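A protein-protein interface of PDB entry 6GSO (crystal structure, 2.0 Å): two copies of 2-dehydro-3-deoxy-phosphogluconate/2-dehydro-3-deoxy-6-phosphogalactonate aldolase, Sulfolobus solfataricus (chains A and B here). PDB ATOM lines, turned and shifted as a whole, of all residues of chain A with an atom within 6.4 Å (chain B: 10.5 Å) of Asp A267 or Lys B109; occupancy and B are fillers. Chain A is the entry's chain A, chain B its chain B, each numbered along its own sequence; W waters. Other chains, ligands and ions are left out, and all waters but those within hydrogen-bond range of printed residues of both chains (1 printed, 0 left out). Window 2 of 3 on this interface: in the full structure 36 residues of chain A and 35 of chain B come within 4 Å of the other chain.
The side-chain amino group of Lys B109 is in salt-bridge range of the side-chain carboxylate of Glu A270 (2.7 Å). OD2 of Asp A267 is in salt-bridge range of NZ of Lys B109 (3.6 Å).
OD1 of Asp A267 is in hydrogen-bond range of N of Glu A270 (2.8 Å). The side-chain carboxylate of Asp A267 sits at hydrogen-bond distance from the backbone NH of Glu A269. O of Lys B113 sits at hydrogen-bond distance from OG1 of Thr B117 (2.9 Å). OG of Ser B107 lies close to N of Lys B109. OG of Ser B107 lies within hydrogen-bond range of N of His B110 (2.8 Å).
Among the printed residues, merely in contact across the chains: Phe A238 with Ser B107, Phe A238 with His B110, Phe A264 with Leu B77, Phe A264 with His B110, Phe A264 with Lys B113 and Phe A264 with Tyr B114.
Printed residues of chain B within 4 Å of Phe A264: Leu B77, His B110, Lys B113 and Tyr B114. Asp A267 touches just one residue of chain B: Lys B109. No residue of chain B comes within 4 Å of Asp A268. Of the printed residues of chain A, Leu B77 touches Phe A264 (3.8 Å). Printed residues of chain A within 4 Å of Lys B109: Asp A267 (3.6 Å) and Glu A270 (2.7 Å). The nearest residue of chain B that does not touch Asp A267 is His B110 (6.1 Å).
Of the 10 printed residues of chain A, 4 touch a printed residue of chain B. Hydrophobic or aromatic side chains of chain A within 4 Å of the printed part of chain B: Phe A264. Of the 20 printed residues of chain B, 6 touch a printed residue of chain A. Among the printed residues, 8 pairs touch across the chains.
No position is printed for both chains.
Water W1 lies within hydrogen-bond range of the backbone carbonyl oxygen of Phe A238 (2.7 Å), the side-chain hydroxyl of Ser B107 (2.8 Å), the side-chain carboxylate of Glu A270 (3.3 Å) and a ring nitrogen (NE2) of His B110 (3.3 Å).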
ATOM      1  N   PHE A 238      -1.969  17.705   4.250  1.00  0.00           N
ATOM      2  CA  PHE A 238      -2.418  16.318   4.331  1.00  0.00           C
ATOM      3  C   PHE A 238      -1.555  15.466   5.247  1.00  0.00           C
ATOM      4  O   PHE A 238      -1.827  14.273   5.384  1.00  0.00           O
ATOM      5  CB  PHE A 238      -2.461  15.708   2.924  1.00  0.00           C
ATOM      6  CG  PHE A 238      -3.350  16.464   1.976  1.00  0.00           C
ATOM      7  CD1 PHE A 238      -4.736  16.445   2.131  1.00  0.00           C
ATOM      8  CD2 PHE A 238      -2.806  17.225   0.960  1.00  0.00           C
ATOM      9  CE1 PHE A 238      -5.554  17.159   1.273  1.00  0.00           C
ATOM     10  CE2 PHE A 238      -3.628  17.942   0.093  1.00  0.00           C
ATOM     11  CZ  PHE A 238      -4.994  17.915   0.257  1.00  0.00           C
ATOM     12  N   PHE A 264       0.175   6.907   6.190  1.00  0.00           N
ATOM     13  CA  PHE A 264      -0.329   6.390   4.926  1.00  0.00           C
ATOM     14  C   PHE A 264       0.134   7.262   3.758  1.00  0.00           C
ATOM     15  O   PHE A 264       0.365   8.468   3.918  1.00  0.00           O
ATOM     16  CB  PHE A 264      -1.861   6.305   4.929  1.00  0.00           C
ATOM     17  CG  PHE A 264      -2.420   5.308   5.895  1.00  0.00           C
ATOM     18  CD1 PHE A 264      -2.472   3.948   5.578  1.00  0.00           C
ATOM     19  CD2 PHE A 264      -2.927   5.725   7.118  1.00  0.00           C
ATOM     20  CE1 PHE A 264      -2.993   3.032   6.475  1.00  0.00           C
ATOM     21  CE2 PHE A 264      -3.458   4.806   8.021  1.00  0.00           C
ATOM     22  CZ  PHE A 264      -3.492   3.457   7.696  1.00  0.00           C
ATOM     23  N   PRO A 265       0.277   6.672   2.571  1.00  0.00           N
ATOM     24  CA  PRO A 265       0.610   7.470   1.390  1.00  0.00           C
ATOM     25  C   PRO A 265      -0.571   8.332   0.974  1.00  0.00           C
ATOM     26  O   PRO A 265      -1.735   7.990   1.203  1.00  0.00           O
ATOM     27  CB  PRO A 265       0.949   6.411   0.334  1.00  0.00           C
ATOM     28  CG  PRO A 265       0.158   5.194   0.768  1.00  0.00           C
ATOM     29  CD  PRO A 265       0.074   5.245   2.248  1.00  0.00           C
ATOM     30  N   LEU A 266      -0.261   9.488   0.395  1.00  0.00           N
ATOM     31  CA  LEU A 266      -1.333  10.357  -0.068  1.00  0.00           C
ATOM     32  C   LEU A 266      -2.062   9.682  -1.219  1.00  0.00           C
ATOM     33  O   LEU A 266      -1.428   9.150  -2.138  1.00  0.00           O
ATOM     34  CB  LEU A 266      -0.791  11.719  -0.508  1.00  0.00           C
ATOM     35  CG  LEU A 266      -0.172  12.615   0.566  1.00  0.00           C
ATOM     36  CD1 LEU A 266       0.017  14.006   0.011  1.00  0.00           C
ATOM     37  CD2 LEU A 266      -1.007  12.663   1.828  1.00  0.00           C
ATOM     38  N   ASP A 267      -3.391   9.687  -1.158  1.00  0.00           N
ATOM     39  CA  ASP A 267      -4.187   9.186  -2.261  1.00  0.00           C
ATOM     40  C   ASP A 267      -4.031  10.127  -3.458  1.00  0.00           C
ATOM     41  O   ASP A 267      -3.342  11.149  -3.401  1.00  0.00           O
ATOM     42  CB  ASP A 267      -5.645   8.972  -1.820  1.00  0.00           C
ATOM     43  CG  ASP A 267      -6.426  10.268  -1.600  1.00  0.00           C
ATOM     44  OD1 ASP A 267      -6.083  11.297  -2.219  1.00  0.00           O
ATOM     45  OD2 ASP A 267      -7.402  10.245  -0.805  1.00  0.00           O
ATOM     46  N   ASP A 268      -4.652   9.760  -4.576  1.00  0.00           N
ATOM     47  CA  ASP A 268      -4.384  10.469  -5.823  1.00  0.00           C
ATOM     48  C   ASP A 268      -5.000  11.867  -5.816  1.00  0.00           C
ATOM     49  O   ASP A 268      -4.413  12.806  -6.373  1.00  0.00           O
ATOM     50  CB  ASP A 268      -4.895   9.632  -6.999  1.00  0.00           C
ATOM     51  CG  ASP A 268      -4.696   8.127  -6.778  1.00  0.00           C
ATOM     52  OD1 ASP A 268      -3.547   7.640  -6.906  1.00  0.00           O
ATOM     53  OD2 ASP A 268      -5.691   7.438  -6.447  1.00  0.00           O
ATOM     54  N   GLU A 269      -6.158  12.037  -5.166  1.00  0.00           N
ATOM     55  CA  GLU A 269      -6.750  13.365  -5.044  1.00  0.00           C
ATOM     56  C   GLU A 269      -5.842  14.291  -4.242  1.00  0.00           C
ATOM     57  O   GLU A 269      -5.503  15.395  -4.692  1.00  0.00           O
ATOM     58  CB  GLU A 269      -8.132  13.257  -4.400  1.00  0.00           C
ATOM     59  CG  GLU A 269      -8.835  14.593  -4.181  1.00  0.00           C
ATOM     60  CD  GLU A 269      -9.304  15.226  -5.477  1.00  0.00           C
ATOM     61  OE1 GLU A 269     -10.023  14.552  -6.247  1.00  0.00           O
ATOM     62  OE2 GLU A 269      -8.943  16.390  -5.738  1.00  0.00           O
ATOM     63  N   GLU A 270      -5.437  13.850  -3.045  1.00  0.00           N
ATOM     64  CA  GLU A 270      -4.548  14.653  -2.209  1.00  0.00           C
ATOM     65  C   GLU A 270      -3.260  14.989  -2.942  1.00  0.00           C
ATOM     66  O   GLU A 270      -2.759  16.119  -2.855  1.00  0.00           O
ATOM     67  CB  GLU A 270      -4.237  13.910  -0.912  1.00  0.00           C
ATOM     68  CG  GLU A 270      -5.441  13.613  -0.043  1.00  0.00           C
ATOM     69  CD  GLU A 270      -5.116  12.677   1.120  1.00  0.00           C
ATOM     70  OE1 GLU A 270      -4.191  11.845   0.975  1.00  0.00           O
ATOM     71  OE2 GLU A 270      -5.784  12.774   2.176  1.00  0.00           O
ATOM     72  N   GLU A 271      -2.711  14.026  -3.680  1.00  0.00           N
ATOM     73  CA  GLU A 271      -1.489  14.273  -4.439  1.00  0.00           C
ATOM     74  C   GLU A 271      -1.698  15.360  -5.486  1.00  0.00           C
ATOM     75  O   GLU A 271      -0.850  16.244  -5.658  1.00  0.00           O
ATOM     76  CB  GLU A 271      -1.015  12.976  -5.102  1.00  0.00           C
ATOM     77  CG  GLU A 271       0.174  13.174  -6.025  1.00  0.00           C
ATOM     78  CD  GLU A 271       0.854  11.868  -6.397  1.00  0.00           C
ATOM     79  OE1 GLU A 271       0.339  10.796  -6.020  1.00  0.00           O
ATOM     80  OE2 GLU A 271       1.911  11.928  -7.054  1.00  0.00           O
ATOM     81  N   ARG A 272      -2.818  15.298  -6.208  1.00  0.00           N
ATOM     82  CA  ARG A 272      -3.145  16.348  -7.164  1.00  0.00           C
ATOM     83  C   ARG A 272      -3.150  17.714  -6.486  1.00  0.00           C
ATOM     84  O   ARG A 272      -2.448  18.639  -6.915  1.00  0.00           O
ATOM     85  CB  ARG A 272      -4.504  16.052  -7.805  1.00  0.00           C
ATOM     86  CG  ARG A 272      -4.629  16.524  -9.255  1.00  0.00           C
ATOM     87  CD  ARG A 272      -5.982  16.159  -9.876  1.00  0.00           C
ATOM     88  NE  ARG A 272      -6.245  14.724  -9.796  1.00  0.00           N
ATOM     89  CZ  ARG A 272      -7.040  14.147  -8.901  1.00  0.00           C
ATOM     90  NH1 ARG A 272      -7.686  14.870  -7.995  1.00  0.00           N
ATOM     91  NH2 ARG A 272      -7.202  12.831  -8.913  1.00  0.00           N
ATOM     92  N   LEU B  77       1.315  -1.002  11.202  1.00  0.00           N
ATOM     93  CA  LEU B  77      -0.063  -1.472  11.159  1.00  0.00           C
ATOM     94  C   LEU B  77      -0.144  -2.963  10.848  1.00  0.00           C
ATOM     95  O   LEU B  77      -1.092  -3.634  11.285  1.00  0.00           O
ATOM     96  CB  LEU B  77      -0.855  -0.657  10.135  1.00  0.00           C
ATOM     97  CG  LEU B  77      -2.312  -1.059   9.957  1.00  0.00           C
ATOM     98  CD1 LEU B  77      -3.016  -1.145  11.286  1.00  0.00           C
ATOM     99  CD2 LEU B  77      -2.945  -0.037   9.067  1.00  0.00           C
ATOM    100  N   PRO B 100      -1.713   6.048  16.999  1.00  0.00           N
ATOM    101  CA  PRO B 100      -0.287   6.110  16.671  1.00  0.00           C
ATOM    102  C   PRO B 100       0.434   7.219  17.408  1.00  0.00           C
ATOM    103  O   PRO B 100       0.144   8.416  17.233  1.00  0.00           O
ATOM    104  CB  PRO B 100      -0.292   6.355  15.155  1.00  0.00           C
ATOM    105  CG  PRO B 100      -1.563   5.705  14.702  1.00  0.00           C
ATOM    106  CD  PRO B 100      -2.550   6.010  15.789  1.00  0.00           C
ATOM    107  N   ARG B 105       0.903  15.899  14.411  1.00  0.00           N
ATOM    108  CA  ARG B 105       0.160  16.373  13.244  1.00  0.00           C
ATOM    109  C   ARG B 105      -0.010  15.262  12.205  1.00  0.00           C
ATOM    110  O   ARG B 105       0.420  15.368  11.053  1.00  0.00           O
ATOM    111  CB  ARG B 105       0.846  17.575  12.599  1.00  0.00           C
ATOM    112  CG  ARG B 105       1.169  18.710  13.506  1.00  0.00           C
ATOM    113  CD  ARG B 105       1.506  19.905  12.641  1.00  0.00           C
ATOM    114  NE  ARG B 105       2.574  20.724  13.204  1.00  0.00           N
ATOM    115  CZ  ARG B 105       2.908  21.929  12.752  1.00  0.00           C
ATOM    116  NH1 ARG B 105       3.902  22.602  13.327  1.00  0.00           N
ATOM    117  NH2 ARG B 105       2.239  22.465  11.735  1.00  0.00           N
ATOM    118  N   MET B 106      -0.610  14.167  12.638  1.00  0.00           N
ATOM    119  CA  MET B 106      -1.171  13.204  11.705  1.00  0.00           C
ATOM    120  C   MET B 106      -2.596  13.631  11.378  1.00  0.00           C
ATOM    121  O   MET B 106      -3.330  14.085  12.260  1.00  0.00           O
ATOM    122  CB  MET B 106      -1.177  11.812  12.306  1.00  0.00           C
ATOM    123  CG  MET B 106       0.158  11.342  12.796  1.00  0.00           C
ATOM    124  SD  MET B 106      -0.003   9.700  13.537  1.00  0.00           S
ATOM    125  CE  MET B 106      -0.801   8.773  12.205  1.00  0.00           C
ATOM    126  N   SER B 107      -2.989  13.487  10.114  1.00  0.00           N
ATOM    127  CA  SER B 107      -4.331  13.899   9.715  1.00  0.00           C
ATOM    128  C   SER B 107      -5.385  13.077  10.446  1.00  0.00           C
ATOM    129  O   SER B 107      -5.194  11.895  10.740  1.00  0.00           O
ATOM    130  CB  SER B 107      -4.507  13.763   8.194  1.00  0.00           C
ATOM    131  OG  SER B 107      -4.674  12.409   7.782  1.00  0.00           O
ATOM    132  N   GLU B 108      -6.517  13.719  10.753  1.00  0.00           N
ATOM    133  CA  GLU B 108      -7.674  12.967  11.215  1.00  0.00           C
ATOM    134  C   GLU B 108      -8.065  11.881  10.217  1.00  0.00           C
ATOM    135  O   GLU B 108      -8.539  10.812  10.617  1.00  0.00           O
ATOM    136  CB  GLU B 108      -8.853  13.907  11.453  1.00  0.00           C
ATOM    137  CG  GLU B 108     -10.077  13.200  12.029  1.00  0.00           C
ATOM    138  CD  GLU B 108     -11.258  14.134  12.257  1.00  0.00           C
ATOM    139  OE1 GLU B 108     -12.406  13.705  12.021  1.00  0.00           O
ATOM    140  OE2 GLU B 108     -11.041  15.283  12.688  1.00  0.00           O
ATOM    141  N   LYS B 109      -7.899  12.149   8.922  1.00  0.00           N
ATOM    142  CA  LYS B 109      -8.181  11.157   7.893  1.00  0.00           C
ATOM    143  C   LYS B 109      -7.390   9.881   8.156  1.00  0.00           C
ATOM    144  O   LYS B 109      -7.956   8.785   8.216  1.00  0.00           O
ATOM    145  CB  LYS B 109      -7.833  11.743   6.522  1.00  0.00           C
ATOM    146  CG  LYS B 109      -8.433  11.031   5.305  1.00  0.00           C
ATOM    147  CD  LYS B 109      -7.817  11.582   4.001  1.00  0.00           C
ATOM    148  CE  LYS B 109      -8.801  11.580   2.832  1.00  0.00           C
ATOM    149  NZ  LYS B 109      -8.405  12.545   1.760  1.00  0.00           N
ATOM    150  N   HIS B 110      -6.077  10.020   8.366  1.00  0.00           N
ATOM    151  CA  HIS B 110      -5.205   8.869   8.596  1.00  0.00           C
ATOM    152  C   HIS B 110      -5.473   8.200   9.942  1.00  0.00           C
ATOM    153  O   HIS B 110      -5.426   6.972  10.044  1.00  0.00           O
ATOM    154  CB  HIS B 110      -3.752   9.313   8.476  1.00  0.00           C
ATOM    155  CG  HIS B 110      -3.360   9.662   7.076  1.00  0.00           C
ATOM    156  ND1 HIS B 110      -2.221  10.375   6.772  1.00  0.00           N
ATOM    157  CD2 HIS B 110      -3.961   9.386   5.894  1.00  0.00           C
ATOM    158  CE1 HIS B 110      -2.132  10.512   5.460  1.00  0.00           C
ATOM    159  NE2 HIS B 110      -3.175   9.917   4.906  1.00  0.00           N
ATOM    160  N   LEU B 111      -5.766   8.983  10.986  1.00  0.00           N
ATOM    161  CA  LEU B 111      -6.124   8.387  12.272  1.00  0.00           C
ATOM    162  C   LEU B 111      -7.385   7.539  12.158  1.00  0.00           C
ATOM    163  O   LEU B 111      -7.455   6.436  12.715  1.00  0.00           O
ATOM    164  CB  LEU B 111      -6.311   9.475  13.326  1.00  0.00           C
ATOM    165  CG  LEU B 111      -5.071  10.326  13.612  1.00  0.00           C
ATOM    166  CD1 LEU B 111      -5.485  11.570  14.357  1.00  0.00           C
ATOM    167  CD2 LEU B 111      -4.047   9.539  14.411  1.00  0.00           C
ATOM    168  N   VAL B 112      -8.388   8.026  11.430  1.00  0.00           N
ATOM    169  CA  VAL B 112      -9.619   7.266  11.263  1.00  0.00           C
ATOM    170  C   VAL B 112      -9.338   5.979  10.507  1.00  0.00           C
ATOM    171  O   VAL B 112      -9.873   4.920  10.842  1.00  0.00           O
ATOM    172  CB  VAL B 112     -10.691   8.117  10.553  1.00  0.00           C
ATOM    173  CG1 VAL B 112     -11.852   7.245  10.074  1.00  0.00           C
ATOM    174  CG2 VAL B 112     -11.205   9.245  11.484  1.00  0.00           C
ATOM    175  N   LYS B 113      -8.528   6.061   9.453  1.00  0.00           N
ATOM    176  CA  LYS B 113      -8.204   4.872   8.678  1.00  0.00           C
ATOM    177  C   LYS B 113      -7.408   3.872   9.504  1.00  0.00           C
ATOM    178  O   LYS B 113      -7.582   2.662   9.340  1.00  0.00           O
ATOM    179  CB  LYS B 113      -7.432   5.256   7.421  1.00  0.00           C
ATOM    180  CG  LYS B 113      -7.188   4.092   6.503  1.00  0.00           C
ATOM    181  CD  LYS B 113      -6.480   4.509   5.229  1.00  0.00           C
ATOM    182  CE  LYS B 113      -6.494   3.378   4.185  1.00  0.00           C
ATOM    183  NZ  LYS B 113      -5.869   3.811   2.899  1.00  0.00           N
ATOM    184  N   TYR B 114      -6.527   4.343  10.389  1.00  0.00           N
ATOM    185  CA  TYR B 114      -5.820   3.415  11.252  1.00  0.00           C
ATOM    186  C   TYR B 114      -6.808   2.579  12.052  1.00  0.00           C
ATOM    187  O   TYR B 114      -6.777   1.347  12.011  1.00  0.00           O
ATOM    188  CB  TYR B 114      -4.866   4.161  12.177  1.00  0.00           C
ATOM    189  CG  TYR B 114      -4.255   3.277  13.244  1.00  0.00           C
ATOM    190  CD1 TYR B 114      -3.184   2.425  12.956  1.00  0.00           C
ATOM    191  CD2 TYR B 114      -4.753   3.286  14.534  1.00  0.00           C
ATOM    192  CE1 TYR B 114      -2.628   1.649  13.926  1.00  0.00           C
ATOM    193  CE2 TYR B 114      -4.209   2.503  15.511  1.00  0.00           C
ATOM    194  CZ  TYR B 114      -3.138   1.680  15.202  1.00  0.00           C
ATOM    195  OH  TYR B 114      -2.588   0.866  16.164  1.00  0.00           O
ATOM    196  N   PHE B 115      -7.711   3.238  12.776  1.00  0.00           N
ATOM    197  CA  PHE B 115      -8.636   2.506  13.642  1.00  0.00           C
ATOM    198  C   PHE B 115      -9.654   1.705  12.842  1.00  0.00           C
ATOM    199  O   PHE B 115     -10.040   0.605  13.247  1.00  0.00           O
ATOM    200  CB  PHE B 115      -9.357   3.469  14.582  1.00  0.00           C
ATOM    201  CG  PHE B 115      -8.504   3.983  15.680  1.00  0.00           C
ATOM    202  CD1 PHE B 115      -8.206   3.180  16.774  1.00  0.00           C
ATOM    203  CD2 PHE B 115      -8.026   5.286  15.641  1.00  0.00           C
ATOM    204  CE1 PHE B 115      -7.436   3.669  17.809  1.00  0.00           C
ATOM    205  CE2 PHE B 115      -7.248   5.776  16.668  1.00  0.00           C
ATOM    206  CZ  PHE B 115      -6.954   4.969  17.753  1.00  0.00           C
ATOM    207  N   LYS B 116     -10.143   2.245  11.734  1.00  0.00           N
ATOM    208  CA  LYS B 116     -11.157   1.506  10.992  1.00  0.00           C
ATOM    209  C   LYS B 116     -10.569   0.223  10.414  1.00  0.00           C
ATOM    210  O   LYS B 116     -11.250  -0.808  10.363  1.00  0.00           O
ATOM    211  CB  LYS B 116     -11.773   2.378   9.895  1.00  0.00           C
ATOM    212  CG  LYS B 116     -13.107   3.012  10.305  1.00  0.00           C
ATOM    213  CD  LYS B 116     -13.749   3.827   9.180  1.00  0.00           C
ATOM    214  CE  LYS B 116     -15.124   4.373   9.600  1.00  0.00           C
ATOM    215  NZ  LYS B 116     -15.818   5.135   8.526  1.00  0.00           N
ATOM    216  N   THR B 117      -9.297   0.257  10.007  1.00  0.00           N
ATOM    217  CA  THR B 117      -8.624  -0.966   9.571  1.00  0.00           C
ATOM    218  C   THR B 117      -8.646  -2.011  10.673  1.00  0.00           C
ATOM    219  O   THR B 117      -8.989  -3.175  10.438  1.00  0.00           O
ATOM    220  CB  THR B 117      -7.183  -0.669   9.159  1.00  0.00           C
ATOM    221  OG1 THR B 117      -7.160   0.123   7.962  1.00  0.00           O
ATOM    222  CG2 THR B 117      -6.405  -1.986   8.918  1.00  0.00           C
ATOM    223  N   ASP B 138      -5.583  13.483  20.506  1.00  0.00           N
ATOM    224  CA  ASP B 138      -6.837  13.123  21.133  1.00  0.00           C
ATOM    225  C   ASP B 138      -7.784  12.568  20.079  1.00  0.00           C
ATOM    226  O   ASP B 138      -7.917  13.125  18.987  1.00  0.00           O
ATOM    227  CB  ASP B 138      -7.426  14.348  21.816  1.00  0.00           C
ATOM    228  CG  ASP B 138      -8.623  14.031  22.656  1.00  0.00           C
ATOM    229  OD1 ASP B 138      -8.642  12.971  23.320  1.00  0.00           O
ATOM    230  OD2 ASP B 138      -9.549  14.881  22.697  1.00  0.00           O
ATOM    231  N   ILE B 139      -8.431  11.478  20.421  1.00  0.00           N
ATOM    232  CA  ILE B 139      -9.517  10.905  19.642  1.00  0.00           C
ATOM    233  C   ILE B 139     -10.753  11.138  20.497  1.00  0.00           C
ATOM    234  O   ILE B 139     -11.079  10.320  21.373  1.00  0.00           O
ATOM    235  CB  ILE B 139      -9.274   9.399  19.355  1.00  0.00           C
ATOM    236  CG1 ILE B 139      -7.866   9.139  18.757  1.00  0.00           C
ATOM    237  CG2 ILE B 139     -10.366   8.840  18.472  1.00  0.00           C
ATOM    238  CD1 ILE B 139      -7.605   9.795  17.449  1.00  0.00           C
ATOM    239  N   VAL B 143     -14.615  12.330  16.851  1.00  0.00           N
ATOM    240  CA  VAL B 143     -13.787  11.418  16.066  1.00  0.00           C
ATOM    241  C   VAL B 143     -14.141   9.972  16.376  1.00  0.00           C
ATOM    242  O   VAL B 143     -14.104   9.109  15.495  1.00  0.00           O
ATOM    243  CB  VAL B 143     -12.294  11.701  16.323  1.00  0.00           C
ATOM    244  CG1 VAL B 143     -11.432  10.771  15.524  1.00  0.00           C
ATOM    245  CG2 VAL B 143     -11.956  13.154  15.976  1.00  0.00           C
ATOM    246  N   GLU B 146     -17.242   9.317  14.383  1.00  0.00           N
ATOM    247  CA  GLU B 146     -16.970   9.225  12.950  1.00  0.00           C
ATOM    248  C   GLU B 146     -16.362   7.866  12.598  1.00  0.00           C
ATOM    249  O   GLU B 146     -16.708   7.262  11.573  1.00  0.00           O
ATOM    250  CB  GLU B 146     -16.042  10.363  12.522  1.00  0.00           C
ATOM    251  CG  GLU B 146     -15.446  10.272  11.104  1.00  0.00           C
ATOM    252  CD  GLU B 146     -16.425  10.661   9.999  1.00  0.00           C
ATOM    253  OE1 GLU B 146     -17.513  11.207  10.305  1.00  0.00           O
ATOM    254  OE2 GLU B 146     -16.095  10.419   8.816  1.00  0.00           O
ATOM    255  N   ILE B 147     -15.459   7.374  13.446  1.00  0.00           N
ATOM    256  CA  ILE B 147     -14.871   6.057  13.241  1.00  0.00           C
ATOM    257  C   ILE B 147     -15.963   4.999  13.288  1.00  0.00           C
ATOM    258  O   ILE B 147     -16.088   4.171  12.383  1.00  0.00           O
ATOM    259  CB  ILE B 147     -13.772   5.799  14.285  1.00  0.00           C
ATOM    260  CG1 ILE B 147     -12.614   6.763  14.029  1.00  0.00           C
ATOM    261  CG2 ILE B 147     -13.308   4.338  14.242  1.00  0.00           C
ATOM    262  CD1 ILE B 147     -11.585   6.795  15.110  1.00  0.00           C
HETATM  263  O   HOH W   1      -4.229  13.087   5.062  1.00  0.00           O
